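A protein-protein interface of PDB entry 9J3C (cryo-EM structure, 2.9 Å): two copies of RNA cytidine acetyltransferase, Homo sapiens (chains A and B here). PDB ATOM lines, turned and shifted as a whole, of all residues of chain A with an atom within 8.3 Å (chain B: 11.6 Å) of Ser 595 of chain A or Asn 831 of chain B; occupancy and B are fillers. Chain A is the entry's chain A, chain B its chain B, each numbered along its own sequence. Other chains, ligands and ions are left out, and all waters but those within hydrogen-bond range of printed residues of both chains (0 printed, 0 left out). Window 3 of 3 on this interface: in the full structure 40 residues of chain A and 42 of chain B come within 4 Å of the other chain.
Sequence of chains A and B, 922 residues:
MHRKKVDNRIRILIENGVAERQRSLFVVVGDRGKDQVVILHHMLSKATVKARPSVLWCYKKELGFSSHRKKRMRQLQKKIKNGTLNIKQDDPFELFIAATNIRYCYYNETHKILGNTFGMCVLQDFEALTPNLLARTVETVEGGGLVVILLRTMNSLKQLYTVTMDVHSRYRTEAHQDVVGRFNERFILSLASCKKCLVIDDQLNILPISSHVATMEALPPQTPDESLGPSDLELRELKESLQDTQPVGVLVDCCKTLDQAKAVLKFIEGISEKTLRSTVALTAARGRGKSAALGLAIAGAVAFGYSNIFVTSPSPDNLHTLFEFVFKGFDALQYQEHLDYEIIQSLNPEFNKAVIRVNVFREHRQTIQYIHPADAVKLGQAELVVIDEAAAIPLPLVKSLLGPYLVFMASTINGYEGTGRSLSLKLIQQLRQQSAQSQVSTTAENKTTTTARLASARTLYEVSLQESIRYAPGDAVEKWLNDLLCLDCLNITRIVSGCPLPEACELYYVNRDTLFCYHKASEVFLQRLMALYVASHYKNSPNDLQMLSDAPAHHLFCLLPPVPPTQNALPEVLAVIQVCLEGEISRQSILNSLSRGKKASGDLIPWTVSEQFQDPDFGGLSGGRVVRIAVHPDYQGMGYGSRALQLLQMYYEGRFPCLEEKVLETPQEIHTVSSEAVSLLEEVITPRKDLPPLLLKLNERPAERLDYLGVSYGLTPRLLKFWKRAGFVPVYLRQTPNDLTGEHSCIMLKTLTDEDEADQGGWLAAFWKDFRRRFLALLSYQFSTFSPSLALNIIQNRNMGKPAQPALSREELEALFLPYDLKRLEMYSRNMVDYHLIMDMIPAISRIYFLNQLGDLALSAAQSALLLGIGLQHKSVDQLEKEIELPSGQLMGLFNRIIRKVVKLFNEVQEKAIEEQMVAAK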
ATOM      1  N   GLN A 588     -15.100  12.604  27.954  1.00  0.00           N
ATOM      2  CA  GLN A 588     -14.883  12.232  26.562  1.00  0.00           C
ATOM      3  C   GLN A 588     -16.113  12.471  25.692  1.00  0.00           C
ATOM      4  O   GLN A 588     -15.977  12.770  24.501  1.00  0.00           O
ATOM      5  CB  GLN A 588     -14.459  10.762  26.470  1.00  0.00           C
ATOM      6  N   SER A 589     -17.317  12.331  26.254  1.00  0.00           N
ATOM      7  CA  SER A 589     -18.526  12.605  25.482  1.00  0.00           C
ATOM      8  C   SER A 589     -18.614  14.078  25.102  1.00  0.00           C
ATOM      9  O   SER A 589     -19.035  14.417  23.989  1.00  0.00           O
ATOM     10  CB  SER A 589     -19.766  12.180  26.269  1.00  0.00           C
ATOM     11  OG  SER A 589     -19.680  10.825  26.670  1.00  0.00           O
ATOM     12  N   ILE A 590     -18.230  14.968  26.020  1.00  0.00           N
ATOM     13  CA  ILE A 590     -18.233  16.397  25.721  1.00  0.00           C
ATOM     14  C   ILE A 590     -17.240  16.711  24.609  1.00  0.00           C
ATOM     15  O   ILE A 590     -17.530  17.501  23.702  1.00  0.00           O
ATOM     16  CB  ILE A 590     -17.935  17.209  26.996  1.00  0.00           C
ATOM     17  CG1 ILE A 590     -19.079  17.063  28.000  1.00  0.00           C
ATOM     18  CG2 ILE A 590     -17.704  18.675  26.659  1.00  0.00           C
ATOM     19  CD1 ILE A 590     -18.862  17.829  29.282  1.00  0.00           C
ATOM     20  N   LEU A 591     -16.056  16.095  24.659  1.00  0.00           N
ATOM     21  CA  LEU A 591     -15.061  16.316  23.615  1.00  0.00           C
ATOM     22  C   LEU A 591     -15.572  15.847  22.259  1.00  0.00           C
ATOM     23  O   LEU A 591     -15.346  16.510  21.239  1.00  0.00           O
ATOM     24  CB  LEU A 591     -13.757  15.605  23.975  1.00  0.00           C
ATOM     25  CG  LEU A 591     -12.950  16.193  25.134  1.00  0.00           C
ATOM     26  CD1 LEU A 591     -11.550  15.597  25.172  1.00  0.00           C
ATOM     27  CD2 LEU A 591     -12.887  17.709  25.032  1.00  0.00           C
ATOM     28  N   ASN A 592     -16.257  14.702  22.225  1.00  0.00           N
ATOM     29  CA  ASN A 592     -16.835  14.224  20.974  1.00  0.00           C
ATOM     30  C   ASN A 592     -17.912  15.176  20.466  1.00  0.00           C
ATOM     31  O   ASN A 592     -17.986  15.457  19.263  1.00  0.00           O
ATOM     32  CB  ASN A 592     -17.407  12.818  21.161  1.00  0.00           C
ATOM     33  CG  ASN A 592     -16.353  11.811  21.574  1.00  0.00           C
ATOM     34  OD1 ASN A 592     -15.212  11.865  21.113  1.00  0.00           O
ATOM     35  ND2 ASN A 592     -16.729  10.885  22.448  1.00  0.00           N
ATOM     36  N   SER A 593     -18.758  15.679  21.368  1.00  0.00           N
ATOM     37  CA  SER A 593     -19.798  16.620  20.962  1.00  0.00           C
ATOM     38  C   SER A 593     -19.200  17.940  20.491  1.00  0.00           C
ATOM     39  O   SER A 593     -19.679  18.531  19.516  1.00  0.00           O
ATOM     40  CB  SER A 593     -20.773  16.853  22.116  1.00  0.00           C
ATOM     41  OG  SER A 593     -21.343  18.148  22.048  1.00  0.00           O
ATOM     42  N   LEU A 594     -18.157  18.421  21.174  1.00  0.00           N
ATOM     43  CA  LEU A 594     -17.507  19.659  20.757  1.00  0.00           C
ATOM     44  C   LEU A 594     -16.853  19.505  19.390  1.00  0.00           C
ATOM     45  O   LEU A 594     -16.901  20.424  18.565  1.00  0.00           O
ATOM     46  CB  LEU A 594     -16.479  20.092  21.801  1.00  0.00           C
ATOM     47  CG  LEU A 594     -17.021  20.661  23.115  1.00  0.00           C
ATOM     48  CD1 LEU A 594     -15.976  21.533  23.794  1.00  0.00           C
ATOM     49  CD2 LEU A 594     -18.306  21.442  22.883  1.00  0.00           C
ATOM     50  N   SER A 595     -16.240  18.348  19.131  1.00  0.00           N
ATOM     51  CA  SER A 595     -15.608  18.094  17.842  1.00  0.00           C
ATOM     52  C   SER A 595     -16.614  17.960  16.707  1.00  0.00           C
ATOM     53  O   SER A 595     -16.206  17.946  15.541  1.00  0.00           O
ATOM     54  CB  SER A 595     -14.748  16.831  17.920  1.00  0.00           C
ATOM     55  OG  SER A 595     -14.000  16.796  19.123  1.00  0.00           O
ATOM     56  N   ARG A 596     -17.902  17.854  17.014  1.00  0.00           N
ATOM     57  CA  ARG A 596     -18.953  17.772  16.008  1.00  0.00           C
ATOM     58  C   ARG A 596     -19.910  18.953  16.047  1.00  0.00           C
ATOM     59  O   ARG A 596     -20.309  19.452  14.992  1.00  0.00           O
ATOM     60  CB  ARG A 596     -19.743  16.464  16.178  1.00  0.00           C
ATOM     61  CG  ARG A 596     -21.040  16.400  15.387  1.00  0.00           C
ATOM     62  CD  ARG A 596     -21.571  14.977  15.312  1.00  0.00           C
ATOM     63  NE  ARG A 596     -20.884  14.086  16.239  1.00  0.00           N
ATOM     64  CZ  ARG A 596     -20.942  12.763  16.188  1.00  0.00           C
ATOM     65  NH1 ARG A 596     -21.651  12.137  15.263  1.00  0.00           N
ATOM     66  NH2 ARG A 596     -20.272  12.049  17.089  1.00  0.00           N
ATOM     67  N   GLY A 597     -20.275  19.424  17.237  1.00  0.00           N
ATOM     68  CA  GLY A 597     -21.169  20.559  17.361  1.00  0.00           C
ATOM     69  C   GLY A 597     -22.630  20.198  17.194  1.00  0.00           C
ATOM     70  O   GLY A 597     -23.306  20.711  16.297  1.00  0.00           O
ATOM     71  N   LYS A 598     -23.133  19.311  18.056  1.00  0.00           N
ATOM     72  CA  LYS A 598     -24.525  18.892  18.006  1.00  0.00           C
ATOM     73  C   LYS A 598     -25.224  18.898  19.358  1.00  0.00           C
ATOM     74  O   LYS A 598     -26.457  18.793  19.387  1.00  0.00           O
ATOM     75  CB  LYS A 598     -24.642  17.485  17.399  1.00  0.00           C
ATOM     76  N   GLU A 611     -20.051  24.395  25.053  1.00  0.00           N
ATOM     77  CA  GLU A 611     -19.938  24.708  23.633  1.00  0.00           C
ATOM     78  C   GLU A 611     -19.439  26.130  23.403  1.00  0.00           C
ATOM     79  O   GLU A 611     -18.687  26.373  22.452  1.00  0.00           O
ATOM     80  CB  GLU A 611     -21.286  24.502  22.941  1.00  0.00           C
ATOM     81  CG  GLU A 611     -21.183  24.225  21.450  1.00  0.00           C
ATOM     82  CD  GLU A 611     -21.773  25.340  20.609  1.00  0.00           C
ATOM     83  OE1 GLU A 611     -22.611  26.101  21.134  1.00  0.00           O
ATOM     84  OE2 GLU A 611     -21.398  25.453  19.423  1.00  0.00           O
ATOM     85  N   GLN A 614     -15.620  26.166  25.357  1.00  0.00           N
ATOM     86  CA  GLN A 614     -14.672  25.090  25.056  1.00  0.00           C
ATOM     87  C   GLN A 614     -13.978  24.588  26.321  1.00  0.00           C
ATOM     88  O   GLN A 614     -12.767  24.364  26.345  1.00  0.00           O
ATOM     89  CB  GLN A 614     -13.648  25.537  24.010  1.00  0.00           C
ATOM     90  CG  GLN A 614     -14.254  26.252  22.814  1.00  0.00           C
ATOM     91  CD  GLN A 614     -14.728  25.292  21.740  1.00  0.00           C
ATOM     92  OE1 GLN A 614     -13.940  24.526  21.186  1.00  0.00           O
ATOM     93  NE2 GLN A 614     -16.021  25.328  21.441  1.00  0.00           N
ATOM     94  N   LEU B 822      -8.202  32.119  19.907  1.00  0.00           N
ATOM     95  CA  LEU B 822      -7.578  31.434  18.779  1.00  0.00           C
ATOM     96  C   LEU B 822      -8.034  29.983  18.697  1.00  0.00           C
ATOM     97  O   LEU B 822      -8.235  29.448  17.601  1.00  0.00           O
ATOM     98  CB  LEU B 822      -6.056  31.515  18.890  1.00  0.00           C
ATOM     99  CG  LEU B 822      -5.452  32.919  18.949  1.00  0.00           C
ATOM    100  CD1 LEU B 822      -4.035  32.871  19.495  1.00  0.00           C
ATOM    101  CD2 LEU B 822      -5.479  33.570  17.576  1.00  0.00           C
ATOM    102  N   LYS B 823      -8.192  29.326  19.850  1.00  0.00           N
ATOM    103  CA  LYS B 823      -8.683  27.953  19.859  1.00  0.00           C
ATOM    104  C   LYS B 823     -10.095  27.871  19.294  1.00  0.00           C
ATOM    105  O   LYS B 823     -10.416  26.944  18.540  1.00  0.00           O
ATOM    106  CB  LYS B 823      -8.639  27.389  21.279  1.00  0.00           C
ATOM    107  CG  LYS B 823      -8.417  25.887  21.344  1.00  0.00           C
ATOM    108  CD  LYS B 823      -7.522  25.512  22.513  1.00  0.00           C
ATOM    109  CE  LYS B 823      -6.141  26.132  22.372  1.00  0.00           C
ATOM    110  NZ  LYS B 823      -5.394  26.125  23.660  1.00  0.00           N
ATOM    111  N   ARG B 824     -10.954  28.829  19.650  1.00  0.00           N
ATOM    112  CA  ARG B 824     -12.307  28.854  19.102  1.00  0.00           C
ATOM    113  C   ARG B 824     -12.286  29.062  17.592  1.00  0.00           C
ATOM    114  O   ARG B 824     -13.043  28.416  16.858  1.00  0.00           O
ATOM    115  CB  ARG B 824     -13.129  29.948  19.782  1.00  0.00           C
ATOM    116  CG  ARG B 824     -13.587  29.599  21.189  1.00  0.00           C
ATOM    117  CD  ARG B 824     -14.127  30.823  21.910  1.00  0.00           C
ATOM    118  NE  ARG B 824     -14.834  31.722  21.005  1.00  0.00           N
ATOM    119  CZ  ARG B 824     -14.866  33.041  21.133  1.00  0.00           C
ATOM    120  NH1 ARG B 824     -14.237  33.655  22.122  1.00  0.00           N
ATOM    121  NH2 ARG B 824     -15.545  33.763  20.246  1.00  0.00           N
ATOM    122  N   LEU B 825     -11.431  29.967  17.110  1.00  0.00           N
ATOM    123  CA  LEU B 825     -11.326  30.197  15.672  1.00  0.00           C
ATOM    124  C   LEU B 825     -10.803  28.960  14.952  1.00  0.00           C
ATOM    125  O   LEU B 825     -11.313  28.591  13.887  1.00  0.00           O
ATOM    126  CB  LEU B 825     -10.425  31.401  15.399  1.00  0.00           C
ATOM    127  CG  LEU B 825     -10.677  32.159  14.094  1.00  0.00           C
ATOM    128  CD1 LEU B 825     -11.880  33.078  14.230  1.00  0.00           C
ATOM    129  CD2 LEU B 825      -9.441  32.945  13.685  1.00  0.00           C
ATOM    130  N   GLU B 826      -9.784  28.308  15.518  1.00  0.00           N
ATOM    131  CA  GLU B 826      -9.279  27.070  14.933  1.00  0.00           C
ATOM    132  C   GLU B 826     -10.331  25.970  14.980  1.00  0.00           C
ATOM    133  O   GLU B 826     -10.480  25.198  14.026  1.00  0.00           O
ATOM    134  CB  GLU B 826      -8.006  26.632  15.659  1.00  0.00           C
ATOM    135  CG  GLU B 826      -7.728  25.135  15.603  1.00  0.00           C
ATOM    136  CD  GLU B 826      -6.686  24.770  14.564  1.00  0.00           C
ATOM    137  OE1 GLU B 826      -6.402  25.609  13.684  1.00  0.00           O
ATOM    138  OE2 GLU B 826      -6.152  23.643  14.628  1.00  0.00           O
ATOM    139  N   MET B 827     -11.076  25.888  16.086  1.00  0.00           N
ATOM    140  CA  MET B 827     -12.104  24.861  16.220  1.00  0.00           C
ATOM    141  C   MET B 827     -13.216  25.058  15.197  1.00  0.00           C
ATOM    142  O   MET B 827     -13.774  24.084  14.680  1.00  0.00           O
ATOM    143  CB  MET B 827     -12.665  24.873  17.641  1.00  0.00           C
ATOM    144  CG  MET B 827     -12.028  23.848  18.568  1.00  0.00           C
ATOM    145  SD  MET B 827     -12.583  22.166  18.246  1.00  0.00           S
ATOM    146  CE  MET B 827     -14.355  22.407  18.275  1.00  0.00           C
ATOM    147  N   TYR B 828     -13.550  26.314  14.893  1.00  0.00           N
ATOM    148  CA  TYR B 828     -14.613  26.597  13.932  1.00  0.00           C
ATOM    149  C   TYR B 828     -14.259  26.082  12.541  1.00  0.00           C
ATOM    150  O   TYR B 828     -15.141  25.664  11.781  1.00  0.00           O
ATOM    151  CB  TYR B 828     -14.886  28.103  13.901  1.00  0.00           C
ATOM    152  CG  TYR B 828     -15.898  28.555  12.870  1.00  0.00           C
ATOM    153  CD1 TYR B 828     -17.062  27.831  12.638  1.00  0.00           C
ATOM    154  CD2 TYR B 828     -15.691  29.712  12.130  1.00  0.00           C
ATOM    155  CE1 TYR B 828     -17.983  28.245  11.696  1.00  0.00           C
ATOM    156  CE2 TYR B 828     -16.608  30.134  11.187  1.00  0.00           C
ATOM    157  CZ  TYR B 828     -17.753  29.397  10.975  1.00  0.00           C
ATOM    158  OH  TYR B 828     -18.670  29.812  10.036  1.00  0.00           O
ATOM    159  N   SER B 829     -12.971  26.087  12.194  1.00  0.00           N
ATOM    160  CA  SER B 829     -12.552  25.766  10.835  1.00  0.00           C
ATOM    161  C   SER B 829     -12.571  24.274  10.525  1.00  0.00           C
ATOM    162  O   SER B 829     -12.366  23.904   9.364  1.00  0.00           O
ATOM    163  CB  SER B 829     -11.150  26.322  10.578  1.00  0.00           C
ATOM    164  OG  SER B 829     -10.156  25.367  10.902  1.00  0.00           O
ATOM    165  N   ARG B 830     -12.808  23.410  11.513  1.00  0.00           N
ATOM    166  CA  ARG B 830     -12.760  21.968  11.294  1.00  0.00           C
ATOM    167  C   ARG B 830     -14.103  21.268  11.436  1.00  0.00           C
ATOM    168  O   ARG B 830     -14.302  20.221  10.819  1.00  0.00           O
ATOM    169  CB  ARG B 830     -11.756  21.318  12.254  1.00  0.00           C
ATOM    170  CG  ARG B 830     -11.581  22.056  13.569  1.00  0.00           C
ATOM    171  CD  ARG B 830     -10.452  21.459  14.391  1.00  0.00           C
ATOM    172  NE  ARG B 830      -9.245  21.261  13.596  1.00  0.00           N
ATOM    173  CZ  ARG B 830      -8.256  20.443  13.927  1.00  0.00           C
ATOM    174  NH1 ARG B 830      -8.293  19.726  15.038  1.00  0.00           N
ATOM    175  NH2 ARG B 830      -7.201  20.343  13.122  1.00  0.00           N
ATOM    176  N   ASN B 831     -15.026  21.813  12.223  1.00  0.00           N
ATOM    177  CA  ASN B 831     -16.362  21.248  12.406  1.00  0.00           C
ATOM    178  C   ASN B 831     -17.417  22.318  12.153  1.00  0.00           C
ATOM    179  O   ASN B 831     -18.327  22.540  12.956  1.00  0.00           O
ATOM    180  CB  ASN B 831     -16.520  20.612  13.788  1.00  0.00           C
ATOM    181  CG  ASN B 831     -16.345  21.602  14.927  1.00  0.00           C
ATOM    182  OD1 ASN B 831     -16.157  22.798  14.713  1.00  0.00           O
ATOM    183  ND2 ASN B 831     -16.421  21.101  16.152  1.00  0.00           N
ATOM    184  N   MET B 832     -17.287  22.982  11.003  1.00  0.00           N
ATOM    185  CA  MET B 832     -17.970  24.223  10.653  1.00  0.00           C
ATOM    186  C   MET B 832     -19.406  24.257  11.157  1.00  0.00           C
ATOM    187  O   MET B 832     -20.218  23.386  10.830  1.00  0.00           O
ATOM    188  CB  MET B 832     -17.942  24.389   9.133  1.00  0.00           C
ATOM    189  CG  MET B 832     -16.575  24.102   8.528  1.00  0.00           C
ATOM    190  SD  MET B 832     -15.459  25.514   8.494  1.00  0.00           S
ATOM    191  CE  MET B 832     -15.227  25.704   6.730  1.00  0.00           C
ATOM    192  N   VAL B 833     -19.714  25.277  11.956  1.00  0.00           N
ATOM    193  CA  VAL B 833     -20.977  25.381  12.677  1.00  0.00           C
ATOM    194  C   VAL B 833     -21.511  26.800  12.537  1.00  0.00           C
ATOM    195  O   VAL B 833     -20.988  27.593  11.747  1.00  0.00           O
ATOM    196  CB  VAL B 833     -20.811  24.994  14.159  1.00  0.00           C
ATOM    197  N   ASP B 834     -22.574  27.115  13.277  1.00  0.00           N
ATOM    198  CA  ASP B 834     -23.144  28.456  13.248  1.00  0.00           C
ATOM    199  C   ASP B 834     -22.082  29.501  13.572  1.00  0.00           C
ATOM    200  O   ASP B 834     -21.252  29.312  14.464  1.00  0.00           O
ATOM    201  CB  ASP B 834     -24.314  28.551  14.234  1.00  0.00           C
ATOM    202  CG  ASP B 834     -23.858  28.644  15.678  1.00  0.00           C
ATOM    203  OD1 ASP B 834     -23.040  27.801  16.101  1.00  0.00           O
ATOM    204  OD2 ASP B 834     -24.320  29.560  16.390  1.00  0.00           O
ATOM    205  N   TYR B 835     -22.106  30.601  12.820  1.00  0.00           N
ATOM    206  CA  TYR B 835     -21.057  31.610  12.880  1.00  0.00           C
ATOM    207  C   TYR B 835     -21.186  32.554  14.068  1.00  0.00           C
ATOM    208  O   TYR B 835     -20.283  33.369  14.286  1.00  0.00           O
ATOM    209  CB  TYR B 835     -21.040  32.422  11.582  1.00  0.00           C
ATOM    210  CG  TYR B 835     -22.347  33.120  11.270  1.00  0.00           C
ATOM    211  CD1 TYR B 835     -23.390  32.443  10.649  1.00  0.00           C
ATOM    212  CD2 TYR B 835     -22.539  34.455  11.597  1.00  0.00           C
ATOM    213  CE1 TYR B 835     -24.584  33.077  10.363  1.00  0.00           C
ATOM    214  CE2 TYR B 835     -23.730  35.098  11.315  1.00  0.00           C
ATOM    215  CZ  TYR B 835     -24.748  34.404  10.698  1.00  0.00           C
ATOM    216  OH  TYR B 835     -25.936  35.040  10.416  1.00  0.00           O
ATOM    217  N   HIS B 836     -22.274  32.471  14.838  1.00  0.00           N
ATOM    218  CA  HIS B 836     -22.457  33.378  15.964  1.00  0.00           C
ATOM    219  C   HIS B 836     -21.433  33.153  17.069  1.00  0.00           C
ATOM    220  O   HIS B 836     -21.234  34.042  17.904  1.00  0.00           O
ATOM    221  CB  HIS B 836     -23.872  33.239  16.529  1.00  0.00           C
ATOM    222  CG  HIS B 836     -24.946  33.654  15.573  1.00  0.00           C
ATOM    223  ND1 HIS B 836     -25.614  32.758  14.767  1.00  0.00           N
ATOM    224  CD2 HIS B 836     -25.468  34.873  15.294  1.00  0.00           C
ATOM    225  CE1 HIS B 836     -26.501  33.406  14.033  1.00  0.00           C
ATOM    226  NE2 HIS B 836     -26.433  34.690  14.334  1.00  0.00           N
ATOM    227  N   LEU B 837     -20.781  31.989  17.095  1.00  0.00           N
ATOM    228  CA  LEU B 837     -19.792  31.719  18.133  1.00  0.00           C
ATOM    229  C   LEU B 837     -18.554  32.594  17.976  1.00  0.00           C
ATOM    230  O   LEU B 837     -17.936  32.976  18.978  1.00  0.00           O
ATOM    231  CB  LEU B 837     -19.405  30.239  18.114  1.00  0.00           C
ATOM    232  CG  LEU B 837     -18.359  29.775  19.130  1.00  0.00           C
ATOM    233  CD1 LEU B 837     -19.030  29.168  20.353  1.00  0.00           C
ATOM    234  CD2 LEU B 837     -17.396  28.783  18.496  1.00  0.00           C
ATOM    235  N   ILE B 838     -18.178  32.926  16.741  1.00  0.00           N
ATOM    236  CA  ILE B 838     -16.958  33.669  16.462  1.00  0.00           C
ATOM    237  C   ILE B 838     -17.240  35.059  15.902  1.00  0.00           C
ATOM    238  O   ILE B 838     -16.356  35.670  15.302  1.00  0.00           O
ATOM    239  CB  ILE B 838     -16.032  32.875  15.518  1.00  0.00           C
ATOM    240  CG1 ILE B 838     -16.735  32.588  14.188  1.00  0.00           C
ATOM    241  CG2 ILE B 838     -15.583  31.581  16.178  1.00  0.00           C
ATOM    242  CD1 ILE B 838     -16.201  33.387  13.021  1.00  0.00           C
ATOM    243  N   MET B 892     -22.065  31.752   2.898  1.00  0.00           N
ATOM    244  CA  MET B 892     -21.508  30.932   3.969  1.00  0.00           C
ATOM    245  C   MET B 892     -20.189  30.298   3.546  1.00  0.00           C
ATOM    246  O   MET B 892     -19.233  30.258   4.329  1.00  0.00           O
ATOM    247  CB  MET B 892     -22.512  29.856   4.383  1.00  0.00           C
ATOM    248  CG  MET B 892     -23.410  30.248   5.545  1.00  0.00           C
ATOM    249  SD  MET B 892     -22.555  31.232   6.790  1.00  0.00           S
ATOM    250  CE  MET B 892     -23.322  32.830   6.544  1.00  0.00           C
ATOM    251  N   ASN B 896     -16.733  31.080   5.267  1.00  0.00           N
ATOM    252  CA  ASN B 896     -16.017  29.960   5.869  1.00  0.00           C
ATOM    253  C   ASN B 896     -14.612  29.829   5.297  1.00  0.00           C
ATOM    254  O   ASN B 896     -13.663  29.519   6.027  1.00  0.00           O
ATOM    255  CB  ASN B 896     -16.806  28.667   5.665  1.00  0.00           C
ATOM    256  CG  ASN B 896     -17.967  28.535   6.632  1.00  0.00           C
ATOM    257  OD1 ASN B 896     -17.772  28.350   7.833  1.00  0.00           O
ATOM    258  ND2 ASN B 896     -19.185  28.628   6.111  1.00  0.00           N
ATOM    259  N   ILE B 899     -12.273  32.172   6.966  1.00  0.00           N
ATOM    260  CA  ILE B 899     -11.896  31.730   8.307  1.00  0.00           C
ATOM    261  C   ILE B 899     -10.747  30.730   8.235  1.00  0.00           C
ATOM    262  O   ILE B 899      -9.785  30.805   9.009  1.00  0.00           O
ATOM    263  CB  ILE B 899     -13.115  31.140   9.039  1.00  0.00           C
ATOM    264  CG1 ILE B 899     -14.139  32.237   9.334  1.00  0.00           C
ATOM    265  CG2 ILE B 899     -12.686  30.451  10.325  1.00  0.00           C
ATOM    266  CD1 ILE B 899     -13.620  33.328  10.243  1.00  0.00           C
ATOM    267  N   ARG B 900     -10.832  29.777   7.301  1.00  0.00           N
ATOM    268  CA  ARG B 900      -9.760  28.798   7.148  1.00  0.00           C
ATOM    269  C   ARG B 900      -8.452  29.466   6.742  1.00  0.00           C
ATOM    270  O   ARG B 900      -7.380  29.099   7.237  1.00  0.00           O
ATOM    271  CB  ARG B 900     -10.159  27.736   6.122  1.00  0.00           C
ATOM    272  CG  ARG B 900     -11.512  27.094   6.380  1.00  0.00           C
ATOM    273  CD  ARG B 900     -11.696  25.846   5.531  1.00  0.00           C
ATOM    274  NE  ARG B 900     -11.062  24.677   6.131  1.00  0.00           N
ATOM    275  CZ  ARG B 900     -11.651  23.499   6.283  1.00  0.00           C
ATOM    276  NH1 ARG B 900     -12.896  23.293   5.885  1.00  0.00           N
ATOM    277  NH2 ARG B 900     -10.974  22.503   6.846  1.00  0.00           N
ATOM    278  N   VAL B 903      -7.160  31.236   9.813  1.00  0.00           N
ATOM    279  CA  VAL B 903      -6.688  30.253  10.783  1.00  0.00           C
ATOM    280  C   VAL B 903      -5.356  29.660  10.342  1.00  0.00           C
ATOM    281  O   VAL B 903      -4.428  29.506  11.147  1.00  0.00           O
ATOM    282  CB  VAL B 903      -7.755  29.162  10.997  1.00  0.00           C
ATOM    283  CG1 VAL B 903      -7.115  27.858  11.448  1.00  0.00           C
ATOM    284  CG2 VAL B 903      -8.793  29.629  12.005  1.00  0.00           C
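The backbone carbonyl oxygen (O) of Leu 594 of chain A sits at hydrogen-bond distance from the side-chain amide nitrogen (ND2) of Asn 831 of chain B, 2.6 Å away. The backbone carbonyl oxygen (O) of Ser 595 of chain A lies close to the side-chain amide nitrogen (ND2) of Asn 831 of chain B (3.2 Å).
Printed residues of chain B within 4 Å of Ser 595 of chain A: Asn 831 (3.2 Å). No residue of chain B comes within 4 Å of Leu 591 of chain A. No residue of chain B comes within 4 Å of Ser 593 of chain A. Leu 594 of chain A touches just these residues of chain B: Met 827 (3.2 Å) and Asn 831 (2.6 Å). No residue of chain B comes within 4 Å of Gly 597 of chain A. Of the printed residues of chain B, Arg 596 of chain A touches Asn 831. Of the printed residues of chain A, Met 827 of chain B touches Leu 594 (3.2 Å) and Gln 614 (3.3 Å). Of the printed residues of chain A, Leu 837 of chain B touches Glu 611 (3.5 Å). Printed residues of chain B within 4 Å of Gln 614 of chain A: Arg 824 and Met 827. Lys 598 of chain A touches none of the printed residues of chain B. The nearest residue of chain B that does not touch Ser 595 of chain A is Met 827 of chain B (4.5 Å). The nearest residue of chain A that does not touch Asn 831 of chain B is Gly 597 of chain A (4.3 Å). The nearest printed residue of chain B that does not touch Gln 614 of chain A is Leu 837 of chain B (4.7 Å).
The backbone carbonyl oxygen (O) of Met 827 of chain B sits close to the side-chain amide oxygen (OD1) of Asn 831 of chain B, at 2.7 Å. The backbone carbonyl oxygen of Glu 611 of chain A sits at hydrogen-bond distance from the side-chain amide nitrogen of Gln 614 of chain A (3.0 Å). O of Leu 591 of chain A lies within hydrogen-bond range of OG of Ser 595 of chain A (2.5 Å). The guanidinium group of Arg 824 of chain B lies within hydrogen-bond range of the backbone carbonyl oxygen of Leu 837 of chain B (2.8 Å).
Met 827 of chain B touches Leu 594 of chain A (CE to O, 3.2 Å). Arg 596 of chain A touches Asn 831 of chain B. Glu 611 of chain A touches Leu 837 of chain B. CG of Gln 614 of chain A touches CG of Arg 824 of chain B, at 3.8 Å. Met 827 of chain B touches Gln 614 of chain A (CG to OE1, 3.3 Å).
No position is printed for both chains. Of the 7 pairs that touch across the chains among the printed residues, none has its exchanged pair printed and touching as well.
Of the 22 printed residues of chain B, 4 touch a printed residue of chain A. Hydrophobic or aromatic side chains of chain B within 4 Å of the printed part of chain A: Met 827 and Leu 837. Of the 13 printed residues of chain A, 5 touch a printed residue of chain B. Along chain A the printed residues that touch a printed residue of chain B span positions 594 to 614. Among the printed residues, 7 pairs touch across the chains. Among the printed residues, no Asp or Glu carboxylate lies within 4 Å of a Lys or Arg side-chain nitrogen of the other chain.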
